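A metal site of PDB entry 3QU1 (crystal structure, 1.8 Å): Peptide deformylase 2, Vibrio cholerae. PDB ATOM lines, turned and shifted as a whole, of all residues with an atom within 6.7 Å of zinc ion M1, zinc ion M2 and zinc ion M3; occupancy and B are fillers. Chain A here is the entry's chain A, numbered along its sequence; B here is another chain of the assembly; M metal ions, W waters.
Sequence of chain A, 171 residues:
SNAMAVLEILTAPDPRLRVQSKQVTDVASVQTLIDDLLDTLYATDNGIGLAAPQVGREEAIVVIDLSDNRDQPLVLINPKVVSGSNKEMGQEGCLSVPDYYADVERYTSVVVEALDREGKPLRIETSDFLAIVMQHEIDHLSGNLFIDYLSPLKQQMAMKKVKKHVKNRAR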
ATOM      1  N   ASP A  45      20.374 -16.904  24.003  1.00  0.00           N
ATOM      2  CA  ASP A  45      21.750 -16.449  24.263  1.00  0.00           C
ATOM      3  C   ASP A  45      22.612 -16.595  23.018  1.00  0.00           C
ATOM      4  O   ASP A  45      23.354 -15.687  22.686  1.00  0.00           O
ATOM      5  CB  ASP A  45      22.392 -17.241  25.412  1.00  0.00           C
ATOM      6  CG  ASP A  45      21.749 -16.982  26.787  1.00  0.00           C
ATOM      7  OD1 ASP A  45      21.273 -15.848  27.087  1.00  0.00           O
ATOM      8  OD2 ASP A  45      21.758 -17.925  27.610  1.00  0.00           O
ATOM      9  N   ASN A  46      22.485 -17.716  22.303  1.00  0.00           N
ATOM     10  CA  ASN A  46      23.336 -17.956  21.130  1.00  0.00           C
ATOM     11  C   ASN A  46      22.742 -18.858  20.046  1.00  0.00           C
ATOM     12  O   ASN A  46      23.457 -19.569  19.337  1.00  0.00           O
ATOM     13  CB  ASN A  46      24.598 -18.616  21.666  1.00  0.00           C
ATOM     14  CG  ASN A  46      24.280 -19.728  22.634  1.00  0.00           C
ATOM     15  OD1 ASN A  46      23.349 -20.500  22.395  1.00  0.00           O
ATOM     16  ND2 ASN A  46      25.003 -19.780  23.771  1.00  0.00           N
ATOM     17  N   PRO A  98      18.500 -28.867  24.852  1.00  0.00           N
ATOM     18  CA  PRO A  98      19.538 -28.035  25.515  1.00  0.00           C
ATOM     19  C   PRO A  98      20.551 -28.803  26.329  1.00  0.00           C
ATOM     20  O   PRO A  98      20.254 -29.790  26.965  1.00  0.00           O
ATOM     21  CB  PRO A  98      18.738 -27.129  26.435  1.00  0.00           C
ATOM     22  CG  PRO A  98      17.456 -27.904  26.710  1.00  0.00           C
ATOM     23  CD  PRO A  98      17.153 -28.595  25.390  1.00  0.00           C
ATOM     24  N   ASP A  99      21.786 -28.336  26.242  1.00  0.00           N
ATOM     25  CA  ASP A  99      22.883 -28.777  27.054  1.00  0.00           C
ATOM     26  C   ASP A  99      23.455 -30.136  26.636  1.00  0.00           C
ATOM     27  O   ASP A  99      24.243 -30.733  27.399  1.00  0.00           O
ATOM     28  CB  ASP A  99      22.501 -28.782  28.529  1.00  0.00           C
ATOM     29  CG  ASP A  99      22.198 -27.406  29.076  1.00  0.00           C
ATOM     30  OD1 ASP A  99      22.123 -26.406  28.298  1.00  0.00           O
ATOM     31  OD2 ASP A  99      21.946 -27.344  30.336  1.00  0.00           O
ATOM     32  N   TYR A 100      23.086 -30.608  25.476  1.00  0.00           N
ATOM     33  CA  TYR A 100      23.679 -31.798  24.899  1.00  0.00           C
ATOM     34  C   TYR A 100      24.294 -31.551  23.543  1.00  0.00           C
ATOM     35  O   TYR A 100      23.675 -31.004  22.636  1.00  0.00           O
ATOM     36  CB  TYR A 100      22.626 -32.901  24.753  1.00  0.00           C
ATOM     37  CG  TYR A 100      23.283 -34.192  24.291  1.00  0.00           C
ATOM     38  CD1 TYR A 100      23.999 -34.982  25.180  1.00  0.00           C
ATOM     39  CD2 TYR A 100      23.258 -34.607  22.946  1.00  0.00           C
ATOM     40  CE1 TYR A 100      24.598 -36.166  24.759  1.00  0.00           C
ATOM     41  CE2 TYR A 100      23.898 -35.772  22.529  1.00  0.00           C
ATOM     42  CZ  TYR A 100      24.560 -36.542  23.410  1.00  0.00           C
ATOM     43  OH  TYR A 100      25.219 -37.698  22.937  1.00  0.00           O
ATOM     44  N   TYR A 101      25.533 -31.920  23.390  1.00  0.00           N
ATOM     45  CA  TYR A 101      26.286 -31.682  22.152  1.00  0.00           C
ATOM     46  C   TYR A 101      26.884 -32.966  21.655  1.00  0.00           C
ATOM     47  O   TYR A 101      27.442 -33.754  22.457  1.00  0.00           O
ATOM     48  CB  TYR A 101      27.429 -30.674  22.368  1.00  0.00           C
ATOM     49  CG  TYR A 101      26.885 -29.344  22.862  1.00  0.00           C
ATOM     50  CD1 TYR A 101      26.301 -28.442  22.022  1.00  0.00           C
ATOM     51  CD2 TYR A 101      26.910 -29.045  24.208  1.00  0.00           C
ATOM     52  CE1 TYR A 101      25.732 -27.229  22.512  1.00  0.00           C
ATOM     53  CE2 TYR A 101      26.420 -27.880  24.691  1.00  0.00           C
ATOM     54  CZ  TYR A 101      25.797 -26.961  23.852  1.00  0.00           C
ATOM     55  OH  TYR A 101      25.251 -25.805  24.468  1.00  0.00           O
ATOM     56  N   LYS A 161      20.240 -35.145  30.236  1.00  0.00           N
ATOM     57  CA  LYS A 161      20.864 -33.823  30.358  1.00  0.00           C
ATOM     58  C   LYS A 161      19.832 -32.721  30.161  1.00  0.00           C
ATOM     59  O   LYS A 161      19.853 -31.709  30.866  1.00  0.00           O
ATOM     60  CB  LYS A 161      21.999 -33.631  29.344  1.00  0.00           C
ATOM     61  CG  LYS A 161      23.194 -34.634  29.461  1.00  0.00           C
ATOM     62  CD  LYS A 161      23.855 -34.746  30.816  1.00  0.00           C
ATOM     63  CE  LYS A 161      24.479 -36.169  31.070  1.00  0.00           C
ATOM     64  NZ  LYS A 161      25.969 -36.181  30.802  1.00  0.00           N
ATOM     65  N   LYS A 164      17.877 -32.485  33.403  1.00  0.00           N
ATOM     66  CA  LYS A 164      18.603 -31.749  34.445  1.00  0.00           C
ATOM     67  C   LYS A 164      18.463 -30.245  34.235  1.00  0.00           C
ATOM     68  O   LYS A 164      18.277 -29.500  35.205  1.00  0.00           O
ATOM     69  CB  LYS A 164      20.082 -32.167  34.611  1.00  0.00           C
ATOM     70  CG  LYS A 164      20.238 -33.567  35.190  1.00  0.00           C
ATOM     71  CD  LYS A 164      21.567 -33.797  35.953  1.00  0.00           C
ATOM     72  CE  LYS A 164      21.798 -35.265  36.363  1.00  0.00           C
ATOM     73  NZ  LYS A 164      22.739 -36.034  35.397  1.00  0.00           N
ATOM     74  N   HIS A 165      18.549 -29.831  32.987  1.00  0.00           N
ATOM     75  CA  HIS A 165      18.532 -28.410  32.661  1.00  0.00           C
ATOM     76  C   HIS A 165      17.161 -27.848  33.014  1.00  0.00           C
ATOM     77  O   HIS A 165      17.007 -26.790  33.648  1.00  0.00           O
ATOM     78  CB  HIS A 165      18.800 -28.264  31.202  1.00  0.00           C
ATOM     79  CG  HIS A 165      18.432 -26.933  30.654  1.00  0.00           C
ATOM     80  ND1 HIS A 165      19.280 -25.848  30.689  1.00  0.00           N
ATOM     81  CD2 HIS A 165      17.309 -26.519  30.010  1.00  0.00           C
ATOM     82  CE1 HIS A 165      18.684 -24.817  30.108  1.00  0.00           C
ATOM     83  NE2 HIS A 165      17.512 -25.211  29.650  1.00  0.00           N
ATOM     84  N   VAL A 166      16.154 -28.592  32.575  1.00  0.00           N
ATOM     85  CA  VAL A 166      14.735 -28.159  32.741  1.00  0.00           C
ATOM     86  C   VAL A 166      14.375 -28.052  34.211  1.00  0.00           C
ATOM     87  O   VAL A 166      13.767 -27.053  34.669  1.00  0.00           O
ATOM     88  CB  VAL A 166      13.791 -29.103  31.950  1.00  0.00           C
ATOM     89  CG1 VAL A 166      12.368 -28.889  32.364  1.00  0.00           C
ATOM     90  CG2 VAL A 166      13.966 -28.855  30.441  1.00  0.00           C
ATOM     91  N   ASN A 168      16.511 -27.801  36.822  1.00  0.00           N
ATOM     92  CA  ASN A 168      17.375 -27.047  37.694  1.00  0.00           C
ATOM     93  C   ASN A 168      16.785 -25.729  38.148  1.00  0.00           C
ATOM     94  O   ASN A 168      16.049 -25.121  37.413  1.00  0.00           O
ATOM     95  CB  ASN A 168      18.698 -26.736  37.043  1.00  0.00           C
ATOM     96  CG  ASN A 168      19.720 -26.298  38.055  1.00  0.00           C
ATOM     97  OD1 ASN A 168      20.117 -27.083  38.930  1.00  0.00           O
ATOM     98  ND2 ASN A 168      20.161 -25.042  37.947  1.00  0.00           N
ATOM     99  N   ARG A 171      21.245 -21.285  39.763  1.00  0.00           N
ATOM    100  CA  ARG A 171      22.254 -20.814  38.803  1.00  0.00           C
ATOM    101  C   ARG A 171      22.691 -19.389  39.230  1.00  0.00           C
ATOM    102  O   ARG A 171      23.564 -19.230  40.110  1.00  0.00           O
ATOM    103  CB  ARG A 171      21.713 -20.778  37.386  1.00  0.00           C
ATOM    104  CG  ARG A 171      21.403 -22.123  36.692  1.00  0.00           C
ATOM    105  CD  ARG A 171      20.921 -21.814  35.285  1.00  0.00           C
ATOM    106  NE  ARG A 171      20.485 -23.008  34.524  1.00  0.00           N
ATOM    107  CZ  ARG A 171      19.347 -23.689  34.728  1.00  0.00           C
ATOM    108  NH1 ARG A 171      18.511 -23.314  35.727  1.00  0.00           N
ATOM    109  NH2 ARG A 171      19.065 -24.757  33.969  1.00  0.00           N
ATOM    110  OXT ARG A 171      22.122 -18.386  38.725  1.00  0.00           O
ATOM    111  N   ASN B  46      17.783 -17.785  32.707  1.00  0.00           N
ATOM    112  CA  ASN B  46      17.276 -18.395  33.931  1.00  0.00           C
ATOM    113  C   ASN B  46      18.158 -18.114  35.148  1.00  0.00           C
ATOM    114  O   ASN B  46      18.053 -18.792  36.155  1.00  0.00           O
ATOM    115  CB  ASN B  46      17.217 -19.924  33.734  1.00  0.00           C
ATOM    116  CG  ASN B  46      18.498 -20.482  33.103  1.00  0.00           C
ATOM    117  OD1 ASN B  46      19.532 -19.780  33.075  1.00  0.00           O
ATOM    118  ND2 ASN B  46      18.447 -21.731  32.571  1.00  0.00           N
ATOM    119  N   PRO B  98      28.622 -23.543  32.488  1.00  0.00           N
ATOM    120  CA  PRO B  98      27.355 -23.765  31.775  1.00  0.00           C
ATOM    121  C   PRO B  98      27.114 -25.225  31.395  1.00  0.00           C
ATOM    122  O   PRO B  98      28.023 -25.934  30.980  1.00  0.00           O
ATOM    123  CB  PRO B  98      27.520 -22.917  30.508  1.00  0.00           C
ATOM    124  CG  PRO B  98      28.972 -22.796  30.297  1.00  0.00           C
ATOM    125  CD  PRO B  98      29.506 -22.665  31.735  1.00  0.00           C
ATOM    126  N   ASP B  99      25.875 -25.639  31.594  1.00  0.00           N
ATOM    127  CA  ASP B  99      25.285 -26.871  31.064  1.00  0.00           C
ATOM    128  C   ASP B  99      25.585 -28.077  31.921  1.00  0.00           C
ATOM    129  O   ASP B  99      25.179 -29.208  31.591  1.00  0.00           O
ATOM    130  CB  ASP B  99      25.696 -27.153  29.622  1.00  0.00           C
ATOM    131  CG  ASP B  99      25.204 -26.153  28.663  1.00  0.00           C
ATOM    132  OD1 ASP B  99      24.573 -25.150  29.011  1.00  0.00           O
ATOM    133  OD2 ASP B  99      25.503 -26.369  27.492  1.00  0.00           O
ATOM    134  N   TYR B 100      26.232 -27.861  33.059  1.00  0.00           N
ATOM    135  CA  TYR B 100      26.622 -28.976  33.929  1.00  0.00           C
ATOM    136  C   TYR B 100      25.886 -28.798  35.264  1.00  0.00           C
ATOM    137  O   TYR B 100      25.974 -27.755  35.879  1.00  0.00           O
ATOM    138  CB  TYR B 100      28.122 -29.003  34.181  1.00  0.00           C
ATOM    139  CG  TYR B 100      28.503 -30.236  34.997  1.00  0.00           C
ATOM    140  CD1 TYR B 100      28.561 -31.484  34.402  1.00  0.00           C
ATOM    141  CD2 TYR B 100      28.668 -30.171  36.356  1.00  0.00           C
ATOM    142  CE1 TYR B 100      28.831 -32.615  35.127  1.00  0.00           C
ATOM    143  CE2 TYR B 100      28.919 -31.310  37.112  1.00  0.00           C
ATOM    144  CZ  TYR B 100      29.013 -32.515  36.498  1.00  0.00           C
ATOM    145  OH  TYR B 100      29.236 -33.647  37.246  1.00  0.00           O
ATOM    146  N   TYR B 101      25.181 -29.830  35.683  1.00  0.00           N
ATOM    147  CA  TYR B 101      24.455 -29.827  36.942  1.00  0.00           C
ATOM    148  C   TYR B 101      24.843 -31.029  37.799  1.00  0.00           C
ATOM    149  O   TYR B 101      25.046 -32.137  37.280  1.00  0.00           O
ATOM    150  CB  TYR B 101      22.935 -29.825  36.650  1.00  0.00           C
ATOM    151  CG  TYR B 101      22.513 -28.740  35.678  1.00  0.00           C
ATOM    152  CD1 TYR B 101      22.274 -27.471  36.114  1.00  0.00           C
ATOM    153  CD2 TYR B 101      22.413 -28.981  34.299  1.00  0.00           C
ATOM    154  CE1 TYR B 101      21.930 -26.441  35.240  1.00  0.00           C
ATOM    155  CE2 TYR B 101      22.086 -27.963  33.405  1.00  0.00           C
ATOM    156  CZ  TYR B 101      21.834 -26.691  33.865  1.00  0.00           C
ATOM    157  OH  TYR B 101      21.533 -25.653  33.023  1.00  0.00           O
ATOM    158  N   LYS B 161      32.076 -30.560  29.372  1.00  0.00           N
ATOM    159  CA  LYS B 161      30.765 -30.040  28.918  1.00  0.00           C
ATOM    160  C   LYS B 161      30.851 -28.553  28.647  1.00  0.00           C
ATOM    161  O   LYS B 161      30.377 -28.075  27.635  1.00  0.00           O
ATOM    162  CB  LYS B 161      29.732 -30.316  29.959  1.00  0.00           C
ATOM    163  CG  LYS B 161      28.380 -29.739  29.670  1.00  0.00           C
ATOM    164  CD  LYS B 161      27.816 -30.036  28.288  1.00  0.00           C
ATOM    165  CE  LYS B 161      27.440 -31.490  28.078  1.00  0.00           C
ATOM    166  NZ  LYS B 161      26.199 -31.945  28.802  1.00  0.00           N
ATOM    167  N   LYS B 164      32.465 -27.980  25.306  1.00  0.00           N
ATOM    168  CA  LYS B 164      31.586 -28.243  24.193  1.00  0.00           C
ATOM    169  C   LYS B 164      30.645 -27.045  23.960  1.00  0.00           C
ATOM    170  O   LYS B 164      30.396 -26.633  22.820  1.00  0.00           O
ATOM    171  CB  LYS B 164      30.761 -29.540  24.396  1.00  0.00           C
ATOM    172  CG  LYS B 164      31.527 -30.840  24.116  1.00  0.00           C
ATOM    173  CD  LYS B 164      30.756 -32.107  24.451  1.00  0.00           C
ATOM    174  CE  LYS B 164      31.679 -33.322  24.571  1.00  0.00           C
ATOM    175  NZ  LYS B 164      30.942 -34.528  25.119  1.00  0.00           N
ATOM    176  N   HIS B 165      30.050 -26.543  25.041  1.00  0.00           N
ATOM    177  CA  HIS B 165      29.111 -25.430  24.975  1.00  0.00           C
ATOM    178  C   HIS B 165      29.833 -24.222  24.362  1.00  0.00           C
ATOM    179  O   HIS B 165      29.333 -23.572  23.465  1.00  0.00           O
ATOM    180  CB  HIS B 165      28.608 -25.124  26.371  1.00  0.00           C
ATOM    181  CG  HIS B 165      27.939 -23.795  26.496  1.00  0.00           C
ATOM    182  ND1 HIS B 165      26.577 -23.610  26.314  1.00  0.00           N
ATOM    183  CD2 HIS B 165      28.453 -22.601  26.836  1.00  0.00           C
ATOM    184  CE1 HIS B 165      26.302 -22.324  26.476  1.00  0.00           C
ATOM    185  NE2 HIS B 165      27.426 -21.692  26.792  1.00  0.00           N
ATOM    186  N   VAL B 166      31.042 -23.964  24.844  1.00  0.00           N
ATOM    187  CA  VAL B 166      31.806 -22.789  24.396  1.00  0.00           C
ATOM    188  C   VAL B 166      32.226 -22.918  22.922  1.00  0.00           C
ATOM    189  O   VAL B 166      32.178 -21.928  22.177  1.00  0.00           O
ATOM    190  CB  VAL B 166      33.011 -22.509  25.361  1.00  0.00           C
ATOM    191  CG1 VAL B 166      33.992 -21.578  24.694  1.00  0.00           C
ATOM    192  CG2 VAL B 166      32.465 -21.928  26.710  1.00  0.00           C
ATOM    193  N   ASN B 168      30.731 -24.856  20.612  1.00  0.00           N
ATOM    194  CA  ASN B 168      29.678 -25.180  19.688  1.00  0.00           C
ATOM    195  C   ASN B 168      29.213 -23.962  18.901  1.00  0.00           C
ATOM    196  O   ASN B 168      29.210 -22.859  19.417  1.00  0.00           O
ATOM    197  CB  ASN B 168      28.458 -25.742  20.415  1.00  0.00           C
ATOM    198  CG  ASN B 168      27.509 -26.392  19.490  1.00  0.00           C
ATOM    199  OD1 ASN B 168      27.840 -27.408  18.882  1.00  0.00           O
ATOM    200  ND2 ASN B 168      26.321 -25.803  19.314  1.00  0.00           N
ATOM    201  N   ARG B 171      23.151 -24.301  16.779  1.00  0.00           N
ATOM    202  CA  ARG B 171      22.026 -24.470  17.721  1.00  0.00           C
ATOM    203  C   ARG B 171      20.769 -24.039  16.976  1.00  0.00           C
ATOM    204  O   ARG B 171      20.706 -22.878  16.540  1.00  0.00           O
ATOM    205  CB  ARG B 171      22.232 -23.598  18.930  1.00  0.00           C
ATOM    206  CG  ARG B 171      23.254 -24.141  19.927  1.00  0.00           C
ATOM    207  CD  ARG B 171      23.359 -23.216  21.089  1.00  0.00           C
ATOM    208  NE  ARG B 171      24.400 -23.599  22.025  1.00  0.00           N
ATOM    209  CZ  ARG B 171      25.702 -23.352  21.893  1.00  0.00           C
ATOM    210  NH1 ARG B 171      26.203 -22.709  20.791  1.00  0.00           N
ATOM    211  NH2 ARG B 171      26.523 -23.739  22.863  1.00  0.00           N
ATOM    212  OXT ARG B 171      19.887 -24.826  16.791  1.00  0.00           O
HETATM  213 ZN    ZN M   1      21.280 -25.734  31.122  1.00  0.00          ZN
HETATM  214 ZN    ZN M   2      22.776 -24.377  28.416  1.00  0.00          ZN
HETATM  215 ZN    ZN M   3      25.191 -25.067  26.086  1.00  0.00          ZN
HETATM  216  O   HOH W   1      20.832 -23.694  27.640  1.00  0.00           O
HETATM  217  O   HOH W   2      23.551 -22.371  28.548  1.00  0.00           O
HETATM  218  O   HOH W   3      22.195 -24.209  30.358  1.00  0.00           O
HETATM  219  O   HOH W   4      23.402 -24.445  26.355  1.00  0.00           O
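Zinc ion M1 is bound by OD2 of Asp 99 of chain A (1.9 Å).
Zinc ion M1 is bound by OH of Tyr 101 of chain B (1.9 Å).
Zinc ion M1 is bound by water W3 (1.9 Å).
A ring nitrogen (ND1) of His 165 of chain A is bound to zinc ion M1 (2.0 Å).
Zinc ion M3 is bound by OH of Tyr 101 of chain A (1.8 Å), water W4 (1.9 Å), OD2 of Asp 99 of chain B (1.9 Å) and ND1 of His 165 of chain B (2.0 Å).
Of the 23 residues printed, 2 come within 4 Å of zinc ion M2.
The nearest printed residue that does not touch zinc ion M2 is His 165 of chain B (4.4 Å).
Residues that only touch zinc ion M1: Arg 171 of chain A.
Of the 23 residues printed, 5 come within 4 Å of zinc ion M1.
The nearest printed residue that does not touch zinc ion M1 is Asn 46 of chain B (5.1 Å).
Merely in contact with zinc ion M3: Arg 171 of chain B (3.7 Å).
Four residues have an atom within 4 Å of zinc ion M3: Tyr 101 of chain A, Asp 99 of chain B, His 165 of chain B and Arg 171 of chain B.
The nearest printed residue that does not touch zinc ion M3 is Asp 99 of chain A (4.01 Å).
OH of Tyr 101 of chain A lies close to NH2 of Arg 171 of chain B, at 2.9 Å.
The side-chain hydroxyl (OH) of Tyr 101 of chain B sits close to the guanidinium group (NH2) of Arg 171 of chain A (2.8 Å).
The backbone carbonyl oxygen (O) of His 165 of chain B lies within hydrogen-bond range of the guanidinium group (NH2) of Arg 171 of chain B, at 2.9 Å.
The backbone carbonyl oxygen (O) of His 165 of chain A sits at hydrogen-bond distance from the guanidinium group (NH2) of Arg 171 of chain A, 2.9 Å away.
The guanidinium group of Arg 171 of chain B lies close to the side-chain amide oxygen of Asn 46 of chain A (3.3 Å).
NH1 of Arg 171 of chain B is in hydrogen-bond range of O of Asn 168 of chain B.
The guanidinium group (NE) of Arg 171 of chain A sits close to the side-chain amide nitrogen (ND2) of Asn 46 of chain B (3.1 Å).
The guanidinium group of Arg 171 of chain A lies close to the side-chain amide nitrogen of Asn 168 of chain A (3.3 Å).
Zinc ion M2 is bound by water W3 (2.0 Å), the side-chain carboxylate of Asp 99 of chain B (2.0 Å), the side-chain carboxylate of Asp 99 of chain A (2.1 Å), water W4 (2.2 Å), water W2 (2.2 Å) and water W1 (2.2 Å).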
